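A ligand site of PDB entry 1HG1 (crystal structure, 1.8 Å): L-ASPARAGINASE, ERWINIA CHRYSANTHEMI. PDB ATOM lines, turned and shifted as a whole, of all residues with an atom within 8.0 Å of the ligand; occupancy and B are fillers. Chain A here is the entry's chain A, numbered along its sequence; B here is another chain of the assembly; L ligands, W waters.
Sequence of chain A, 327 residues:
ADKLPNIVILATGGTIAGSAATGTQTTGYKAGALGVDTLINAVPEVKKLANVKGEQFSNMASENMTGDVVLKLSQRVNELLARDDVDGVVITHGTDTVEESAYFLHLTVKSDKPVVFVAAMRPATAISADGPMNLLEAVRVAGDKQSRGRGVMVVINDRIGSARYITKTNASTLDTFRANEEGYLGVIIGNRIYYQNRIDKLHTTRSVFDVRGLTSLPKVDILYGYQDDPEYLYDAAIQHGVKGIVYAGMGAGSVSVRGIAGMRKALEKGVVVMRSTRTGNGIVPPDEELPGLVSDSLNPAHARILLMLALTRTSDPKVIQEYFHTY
The side-chain hydroxyl (OG) of Ser 62 sits at hydrogen-bond distance from an oxygen (O1) of the ligand. N of Ser 62 sits at hydrogen-bond distance from O3 of the ligand, 2.8 Å away. An oxygen (O1) of the ligand lies within hydrogen-bond range of the backbone NH of Asp 96, at 3.0 Å. The side-chain hydroxyl (OG1) of Thr 15 lies close to an oxygen (O4) of the ligand (3.3 Å). The backbone NH (N) of Gly 14 sits close to an oxygen (O2) of the ligand (3.3 Å). OE1 of Glu 63 lies within salt-bridge range of N1 of the ligand, 2.8 Å away. N of Thr 15 is in hydrogen-bond range of O2 of the ligand, 3.5 Å away. OG1 of Thr 95 sits at hydrogen-bond distance from O4 of the ligand (3.4 Å). The backbone NH of Thr 95 sits at hydrogen-bond distance from an oxygen (O4) of the ligand (2.8 Å). The side-chain carboxylate (OD2) of Asp 96 lies within salt-bridge range of a nitrogen (N1) of the ligand (2.7 Å).
The side-chain hydroxyl of Ser 254 of chain B sits close to the backbone carbonyl oxygen of Met 250 of chain B, at 3.4 Å. The side-chain hydroxyl (OG) of Ser 62 lies close to the backbone NH (N) of Asp 96 (3.3 Å). The backbone carbonyl oxygen (O) of Ser 62 sits at hydrogen-bond distance from the side-chain hydroxyl (OG1) of Thr 97, 2.7 Å away. The side-chain hydroxyl (OG1) of Thr 95 lies within hydrogen-bond range of the side-chain sulfur (SD) of Met 121, 3.5 Å away. OD2 of Asp 96 sits at hydrogen-bond distance from OG of Ser 254 of chain B (2.5 Å). The side-chain carboxylate (OD1) of Asp 96 is in salt-bridge range of the side-chain amino group (NZ) of Lys 168, at 2.8 Å. OG1 of Thr 95 lies within hydrogen-bond range of NZ of Lys 168 (2.8 Å).
Residues that only touch the ligand: Gly 94 (3.2 Å), Ala 61 (3.2 Å) and Ser 254 of chain B (3.995 Å). Within 4 Å of the ligand: Gly 14, Thr 15, Ala 61, Ser 62, Glu 63, Gly 94, Thr 95, Asp 96 and Ser 254 of chain B. The nearest printed residue that does not touch the ligand is Ala 120 (4.4 Å).
Water W4 lies within hydrogen-bond range of an oxygen (O4) of the ligand, the side-chain hydroxyl (OG1) of Thr 95, the backbone carbonyl oxygen (O) of Ala 120 and the side-chain hydroxyl (OG1) of Thr 15. Water W1 lies within hydrogen-bond range of the backbone carbonyl oxygen (O) of Met 60, the backbone NH (N) of Gly 14, an oxygen (O3) of the ligand and the backbone NH (N) of Ser 62. Water W2 lies within hydrogen-bond range of O2 of the ligand (2.8 Å) and N of Gly 14 (3.2 Å). Water W3 lies within hydrogen-bond range of OE2 of Glu 63 (2.6 Å) and N1 of the ligand (2.9 Å).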
ATOM      1  N   THR A  12      -2.466  21.250  23.792  1.00  0.00           N
ATOM      2  CA  THR A  12      -1.505  22.076  24.526  1.00  0.00           C
ATOM      3  C   THR A  12      -0.645  22.844  23.532  1.00  0.00           C
ATOM      4  O   THR A  12      -0.012  23.837  23.873  1.00  0.00           O
ATOM      5  CB  THR A  12      -0.566  21.219  25.403  1.00  0.00           C
ATOM      6  OG1 THR A  12       0.306  20.446  24.568  1.00  0.00           O
ATOM      7  CG2 THR A  12      -1.374  20.277  26.288  1.00  0.00           C
ATOM      8  N   GLY A  13      -0.643  22.368  22.291  1.00  0.00           N
ATOM      9  CA  GLY A  13       0.149  22.980  21.236  1.00  0.00           C
ATOM     10  C   GLY A  13       0.909  21.896  20.498  1.00  0.00           C
ATOM     11  O   GLY A  13       0.606  20.707  20.640  1.00  0.00           O
ATOM     12  N   GLY A  14       1.892  22.283  19.698  1.00  0.00           N
ATOM     13  CA  GLY A  14       2.680  21.300  18.968  1.00  0.00           C
ATOM     14  C   GLY A  14       2.574  21.366  17.460  1.00  0.00           C
ATOM     15  O   GLY A  14       1.655  21.977  16.906  1.00  0.00           O
ATOM     16  N   THR A  15       3.521  20.727  16.790  1.00  0.00           N
ATOM     17  CA  THR A  15       3.577  20.694  15.341  1.00  0.00           C
ATOM     18  C   THR A  15       2.321  20.029  14.765  1.00  0.00           C
ATOM     19  O   THR A  15       2.002  20.189  13.588  1.00  0.00           O
ATOM     20  CB  THR A  15       4.832  19.935  14.860  1.00  0.00           C
ATOM     21  OG1 THR A  15       6.015  20.626  15.297  1.00  0.00           O
ATOM     22  CG2 THR A  15       4.865  19.822  13.353  1.00  0.00           C
ATOM     23  N   ILE A  16       1.601  19.291  15.611  1.00  0.00           N
ATOM     24  CA  ILE A  16       0.385  18.587  15.202  1.00  0.00           C
ATOM     25  C   ILE A  16      -0.814  19.516  15.061  1.00  0.00           C
ATOM     26  O   ILE A  16      -1.495  19.428  14.013  1.00  0.00           O
ATOM     27  CB  ILE A  16       0.040  17.454  16.200  1.00  0.00           C
ATOM     28  CG1 ILE A  16      -1.203  16.701  15.714  1.00  0.00           C
ATOM     29  CG2 ILE A  16      -0.192  18.042  17.587  1.00  0.00           C
ATOM     30  CD1 ILE A  16      -1.505  15.451  16.530  1.00  0.00           C
ATOM     31  OXT ILE A  16      -1.081  20.296  15.995  1.00  0.00           O
ATOM     32  N   ASN A  59      -1.572  26.702  24.330  1.00  0.00           N
ATOM     33  CA  ASN A  59      -1.068  26.781  22.959  1.00  0.00           C
ATOM     34  C   ASN A  59       0.355  27.310  22.938  1.00  0.00           C
ATOM     35  O   ASN A  59       0.579  28.518  22.808  1.00  0.00           O
ATOM     36  CB  ASN A  59      -1.977  27.671  22.114  1.00  0.00           C
ATOM     37  CG  ASN A  59      -1.483  27.794  20.675  1.00  0.00           C
ATOM     38  OD1 ASN A  59      -1.300  26.787  19.989  1.00  0.00           O
ATOM     39  ND2 ASN A  59      -1.278  29.021  20.220  1.00  0.00           N
ATOM     40  N   MET A  60       1.312  26.406  23.066  1.00  0.00           N
ATOM     41  CA  MET A  60       2.722  26.785  23.064  1.00  0.00           C
ATOM     42  C   MET A  60       3.558  25.616  22.573  1.00  0.00           C
ATOM     43  O   MET A  60       3.136  24.458  22.653  1.00  0.00           O
ATOM     44  CB  MET A  60       3.165  27.165  24.474  1.00  0.00           C
ATOM     45  CG  MET A  60       3.151  25.999  25.440  1.00  0.00           C
ATOM     46  SD  MET A  60       3.683  26.434  27.108  1.00  0.00           S
ATOM     47  CE  MET A  60       2.095  26.790  27.874  1.00  0.00           C
ATOM     48  N   ALA A  61       4.743  25.920  22.064  1.00  0.00           N
ATOM     49  CA  ALA A  61       5.649  24.879  21.594  1.00  0.00           C
ATOM     50  C   ALA A  61       6.036  24.082  22.837  1.00  0.00           C
ATOM     51  O   ALA A  61       6.144  24.651  23.914  1.00  0.00           O
ATOM     52  CB  ALA A  61       6.867  25.502  20.948  1.00  0.00           C
ATOM     53  N   SER A  62       6.222  22.773  22.696  1.00  0.00           N
ATOM     54  CA  SER A  62       6.567  21.950  23.844  1.00  0.00           C
ATOM     55  C   SER A  62       7.875  22.348  24.533  1.00  0.00           C
ATOM     56  O   SER A  62       8.057  22.060  25.711  1.00  0.00           O
ATOM     57  CB  SER A  62       6.602  20.460  23.470  1.00  0.00           C
ATOM     58  OG  SER A  62       7.703  20.147  22.638  1.00  0.00           O
ATOM     59  N   GLU A  63       8.782  23.001  23.804  1.00  0.00           N
ATOM     60  CA  GLU A  63      10.034  23.407  24.433  1.00  0.00           C
ATOM     61  C   GLU A  63       9.791  24.478  25.490  1.00  0.00           C
ATOM     62  O   GLU A  63      10.693  24.815  26.244  1.00  0.00           O
ATOM     63  CB  GLU A  63      11.029  23.937  23.399  1.00  0.00           C
ATOM     64  CG  GLU A  63      10.572  25.183  22.664  1.00  0.00           C
ATOM     65  CD  GLU A  63       9.965  24.861  21.315  1.00  0.00           C
ATOM     66  OE1 GLU A  63       9.234  23.851  21.221  1.00  0.00           O
ATOM     67  OE2 GLU A  63      10.230  25.618  20.357  1.00  0.00           O
ATOM     68  N   ASN A  64       8.568  24.994  25.539  1.00  0.00           N
ATOM     69  CA  ASN A  64       8.223  26.015  26.521  1.00  0.00           C
ATOM     70  C   ASN A  64       7.291  25.504  27.626  1.00  0.00           C
ATOM     71  O   ASN A  64       6.917  26.254  28.522  1.00  0.00           O
ATOM     72  CB  ASN A  64       7.583  27.232  25.830  1.00  0.00           C
ATOM     73  CG  ASN A  64       8.620  28.152  25.200  1.00  0.00           C
ATOM     74  OD1 ASN A  64       9.591  28.554  25.860  1.00  0.00           O
ATOM     75  ND2 ASN A  64       8.429  28.495  23.925  1.00  0.00           N
ATOM     76  N   MET A  65       6.919  24.229  27.546  1.00  0.00           N
ATOM     77  CA  MET A  65       6.079  23.640  28.581  1.00  0.00           C
ATOM     78  C   MET A  65       6.860  23.700  29.887  1.00  0.00           C
ATOM     79  O   MET A  65       8.056  23.411  29.909  1.00  0.00           O
ATOM     80  CB  MET A  65       5.756  22.173  28.253  1.00  0.00           C
ATOM     81  CG  MET A  65       4.511  21.968  27.410  1.00  0.00           C
ATOM     82  SD  MET A  65       2.993  22.397  28.298  1.00  0.00           S
ATOM     83  CE  MET A  65       2.230  23.469  27.136  1.00  0.00           C
ATOM     84  N   HIS A  93       0.360  17.277  21.970  1.00  0.00           N
ATOM     85  CA  HIS A  93       1.520  17.910  22.561  1.00  0.00           C
ATOM     86  C   HIS A  93       2.661  17.958  21.542  1.00  0.00           C
ATOM     87  O   HIS A  93       2.663  17.212  20.559  1.00  0.00           O
ATOM     88  CB  HIS A  93       1.914  17.075  23.780  1.00  0.00           C
ATOM     89  CG  HIS A  93       2.861  17.735  24.725  1.00  0.00           C
ATOM     90  ND1 HIS A  93       4.208  17.871  24.463  1.00  0.00           N
ATOM     91  CD2 HIS A  93       2.681  18.216  25.980  1.00  0.00           C
ATOM     92  CE1 HIS A  93       4.807  18.406  25.503  1.00  0.00           C
ATOM     93  NE2 HIS A  93       3.909  18.623  26.441  1.00  0.00           N
ATOM     94  N   GLY A  94       3.634  18.837  21.770  1.00  0.00           N
ATOM     95  CA  GLY A  94       4.770  18.917  20.864  1.00  0.00           C
ATOM     96  C   GLY A  94       5.631  17.701  21.129  1.00  0.00           C
ATOM     97  O   GLY A  94       5.608  17.156  22.238  1.00  0.00           O
ATOM     98  N   THR A  95       6.387  17.247  20.136  1.00  0.00           N
ATOM     99  CA  THR A  95       7.233  16.069  20.297  1.00  0.00           C
ATOM    100  C   THR A  95       8.464  16.295  21.179  1.00  0.00           C
ATOM    101  O   THR A  95       8.903  15.383  21.884  1.00  0.00           O
ATOM    102  CB  THR A  95       7.735  15.544  18.938  1.00  0.00           C
ATOM    103  OG1 THR A  95       8.490  16.580  18.296  1.00  0.00           O
ATOM    104  CG2 THR A  95       6.570  15.147  18.037  1.00  0.00           C
ATOM    105  N   ASP A  96       9.010  17.508  21.147  1.00  0.00           N
ATOM    106  CA  ASP A  96      10.224  17.816  21.901  1.00  0.00           C
ATOM    107  C   ASP A  96      10.247  17.457  23.387  1.00  0.00           C
ATOM    108  O   ASP A  96      11.246  16.932  23.867  1.00  0.00           O
ATOM    109  CB  ASP A  96      10.592  19.298  21.739  1.00  0.00           C
ATOM    110  CG  ASP A  96      10.902  19.672  20.294  1.00  0.00           C
ATOM    111  OD1 ASP A  96      11.116  18.750  19.466  1.00  0.00           O
ATOM    112  OD2 ASP A  96      10.950  20.880  19.997  1.00  0.00           O
ATOM    113  N   THR A  97       9.171  17.759  24.122  1.00  0.00           N
ATOM    114  CA  THR A  97       9.164  17.437  25.544  1.00  0.00           C
ATOM    115  C   THR A  97       7.972  16.590  25.981  1.00  0.00           C
ATOM    116  O   THR A  97       7.641  16.518  27.158  1.00  0.00           O
ATOM    117  CB  THR A  97       9.190  18.720  26.413  1.00  0.00           C
ATOM    118  OG1 THR A  97       7.952  19.419  26.281  1.00  0.00           O
ATOM    119  CG2 THR A  97      10.340  19.630  25.988  1.00  0.00           C
ATOM    120  N   VAL A  98       7.343  15.931  25.015  1.00  0.00           N
ATOM    121  CA  VAL A  98       6.195  15.097  25.338  1.00  0.00           C
ATOM    122  C   VAL A  98       6.565  13.999  26.344  1.00  0.00           C
ATOM    123  O   VAL A  98       5.752  13.619  27.187  1.00  0.00           O
ATOM    124  CB  VAL A  98       5.576  14.464  24.065  1.00  0.00           C
ATOM    125  CG1 VAL A  98       6.507  13.411  23.474  1.00  0.00           C
ATOM    126  CG2 VAL A  98       4.212  13.864  24.394  1.00  0.00           C
ATOM    127  N   ALA A 119       1.411  13.260  19.258  1.00  0.00           N
ATOM    128  CA  ALA A 119       2.187  14.354  18.675  1.00  0.00           C
ATOM    129  C   ALA A 119       2.427  14.086  17.196  1.00  0.00           C
ATOM    130  O   ALA A 119       1.944  13.098  16.656  1.00  0.00           O
ATOM    131  CB  ALA A 119       3.531  14.483  19.411  1.00  0.00           C
ATOM    132  N   ALA A 120       3.163  14.980  16.556  1.00  0.00           N
ATOM    133  CA  ALA A 120       3.468  14.846  15.138  1.00  0.00           C
ATOM    134  C   ALA A 120       4.825  15.470  14.812  1.00  0.00           C
ATOM    135  O   ALA A 120       5.123  16.592  15.224  1.00  0.00           O
ATOM    136  CB  ALA A 120       2.375  15.498  14.297  1.00  0.00           C
ATOM    137  N   MET A 121       5.652  14.730  14.068  1.00  0.00           N
ATOM    138  CA  MET A 121       6.971  15.189  13.678  1.00  0.00           C
ATOM    139  C   MET A 121       6.958  16.136  12.476  1.00  0.00           C
ATOM    140  O   MET A 121       7.917  16.857  12.237  1.00  0.00           O
ATOM    141  CB  MET A 121       7.879  13.985  13.405  1.00  0.00           C
ATOM    142  CG  MET A 121       8.407  13.334  14.678  1.00  0.00           C
ATOM    143  SD  MET A 121       9.409  14.516  15.634  1.00  0.00           S
ATOM    144  CE  MET A 121      10.946  14.466  14.716  1.00  0.00           C
ATOM    145  N   ARG A 122       5.863  16.128  11.724  1.00  0.00           N
ATOM    146  CA  ARG A 122       5.728  17.002  10.569  1.00  0.00           C
ATOM    147  C   ARG A 122       4.562  17.955  10.771  1.00  0.00           C
ATOM    148  O   ARG A 122       3.537  17.571  11.327  1.00  0.00           O
ATOM    149  CB  ARG A 122       5.496  16.196   9.290  1.00  0.00           C
ATOM    150  CG  ARG A 122       6.717  15.436   8.807  1.00  0.00           C
ATOM    151  CD  ARG A 122       6.353  14.521   7.642  1.00  0.00           C
ATOM    152  NE  ARG A 122       7.509  13.812   7.113  1.00  0.00           N
ATOM    153  CZ  ARG A 122       7.436  12.815   6.245  1.00  0.00           C
ATOM    154  NH1 ARG A 122       6.258  12.394   5.808  1.00  0.00           N
ATOM    155  NH2 ARG A 122       8.548  12.228   5.807  1.00  0.00           N
ATOM    156  N   LYS A 168      12.218  10.646  22.689  1.00  0.00           N
ATOM    157  CA  LYS A 168      12.484  11.101  21.324  1.00  0.00           C
ATOM    158  C   LYS A 168      13.975  10.838  21.098  1.00  0.00           C
ATOM    159  O   LYS A 168      14.824  11.513  21.683  1.00  0.00           O
ATOM    160  CB  LYS A 168      12.172  12.599  21.193  1.00  0.00           C
ATOM    161  CG  LYS A 168      12.255  13.105  19.761  1.00  0.00           C
ATOM    162  CD  LYS A 168      11.802  14.549  19.648  1.00  0.00           C
ATOM    163  CE  LYS A 168      11.853  15.026  18.200  1.00  0.00           C
ATOM    164  NZ  LYS A 168      11.245  16.384  18.056  1.00  0.00           N
ATOM    165  N   PHE A 177      10.405   8.252  18.145  1.00  0.00           N
ATOM    166  CA  PHE A 177      10.072   7.703  19.459  1.00  0.00           C
ATOM    167  C   PHE A 177      10.295   6.201  19.558  1.00  0.00           C
ATOM    168  O   PHE A 177       9.661   5.427  18.839  1.00  0.00           O
ATOM    169  CB  PHE A 177       8.637   8.061  19.847  1.00  0.00           C
ATOM    170  CG  PHE A 177       8.461   9.524  20.147  1.00  0.00           C
ATOM    171  CD1 PHE A 177       8.185  10.420  19.122  1.00  0.00           C
ATOM    172  CD2 PHE A 177       8.644  10.012  21.440  1.00  0.00           C
ATOM    173  CE1 PHE A 177       8.099  11.795  19.381  1.00  0.00           C
ATOM    174  CE2 PHE A 177       8.558  11.373  21.704  1.00  0.00           C
ATOM    175  CZ  PHE A 177       8.279  12.274  20.670  1.00  0.00           C
ATOM    176  N   MET B 250      16.262  20.229  23.049  1.00  0.00           N
ATOM    177  CA  MET B 250      15.042  19.447  23.011  1.00  0.00           C
ATOM    178  C   MET B 250      14.761  19.261  21.533  1.00  0.00           C
ATOM    179  O   MET B 250      14.832  20.215  20.755  1.00  0.00           O
ATOM    180  CB  MET B 250      13.912  20.217  23.694  1.00  0.00           C
ATOM    181  CG  MET B 250      14.128  20.426  25.193  1.00  0.00           C
ATOM    182  SD  MET B 250      13.057  21.671  25.965  1.00  0.00           S
ATOM    183  CE  MET B 250      14.040  23.161  25.736  1.00  0.00           C
ATOM    184  N   GLY B 251      14.455  18.032  21.138  1.00  0.00           N
ATOM    185  CA  GLY B 251      14.175  17.763  19.745  1.00  0.00           C
ATOM    186  C   GLY B 251      15.281  18.262  18.835  1.00  0.00           C
ATOM    187  O   GLY B 251      16.475  18.080  19.113  1.00  0.00           O
ATOM    188  N   ALA B 252      14.883  18.891  17.731  1.00  0.00           N
ATOM    189  CA  ALA B 252      15.834  19.410  16.753  1.00  0.00           C
ATOM    190  C   ALA B 252      16.460  20.727  17.185  1.00  0.00           C
ATOM    191  O   ALA B 252      16.368  21.727  16.472  1.00  0.00           O
ATOM    192  CB  ALA B 252      15.141  19.567  15.402  1.00  0.00           C
ATOM    193  N   SER B 254      15.549  22.678  19.525  1.00  0.00           N
ATOM    194  CA  SER B 254      14.527  23.652  19.891  1.00  0.00           C
ATOM    195  C   SER B 254      14.961  24.365  21.162  1.00  0.00           C
ATOM    196  O   SER B 254      15.541  23.756  22.063  1.00  0.00           O
ATOM    197  CB  SER B 254      13.191  22.944  20.107  1.00  0.00           C
ATOM    198  OG  SER B 254      12.799  22.256  18.930  1.00  0.00           O
ATOM    199  N   VAL B 255      14.663  25.654  21.245  1.00  0.00           N
ATOM    200  CA  VAL B 255      15.060  26.466  22.392  1.00  0.00           C
ATOM    201  C   VAL B 255      13.882  27.166  23.088  1.00  0.00           C
ATOM    202  O   VAL B 255      13.028  27.756  22.431  1.00  0.00           O
ATOM    203  CB  VAL B 255      16.066  27.538  21.958  1.00  0.00           C
ATOM    204  CG1 VAL B 255      16.736  28.145  23.177  1.00  0.00           C
ATOM    205  CG2 VAL B 255      17.106  26.939  21.019  1.00  0.00           C
HETATM  206  N1  LIG L   1       8.804  22.206  18.951  1.00  0.00           N
HETATM  207  C1  LIG L   1       7.899  21.397  18.137  1.00  0.00           C
HETATM  208  C2  LIG L   1       7.413  20.186  18.916  1.00  0.00           C
HETATM  209  O1  LIG L   1       7.813  20.057  20.094  1.00  0.00           O
HETATM  210  C3  LIG L   1       6.698  22.241  17.692  1.00  0.00           C
HETATM  211  C4  LIG L   1       5.775  22.601  18.843  1.00  0.00           C
HETATM  212  O2  LIG L   1       4.808  23.362  18.608  1.00  0.00           O
HETATM  213  O3  LIG L   1       6.012  22.133  19.978  1.00  0.00           O
HETATM  214  O4  LIG L   1       6.645  19.385  18.332  1.00  0.00           O
HETATM  215  O   HOH W   1       3.739  22.466  21.428  1.00  0.00           O
HETATM  216  O   HOH W   2       2.851  25.242  19.064  1.00  0.00           O
HETATM  217  O   HOH W   3       9.410  24.893  18.017  1.00  0.00           O
HETATM  218  O   HOH W   4       7.372  17.983  16.400  1.00  0.00           O
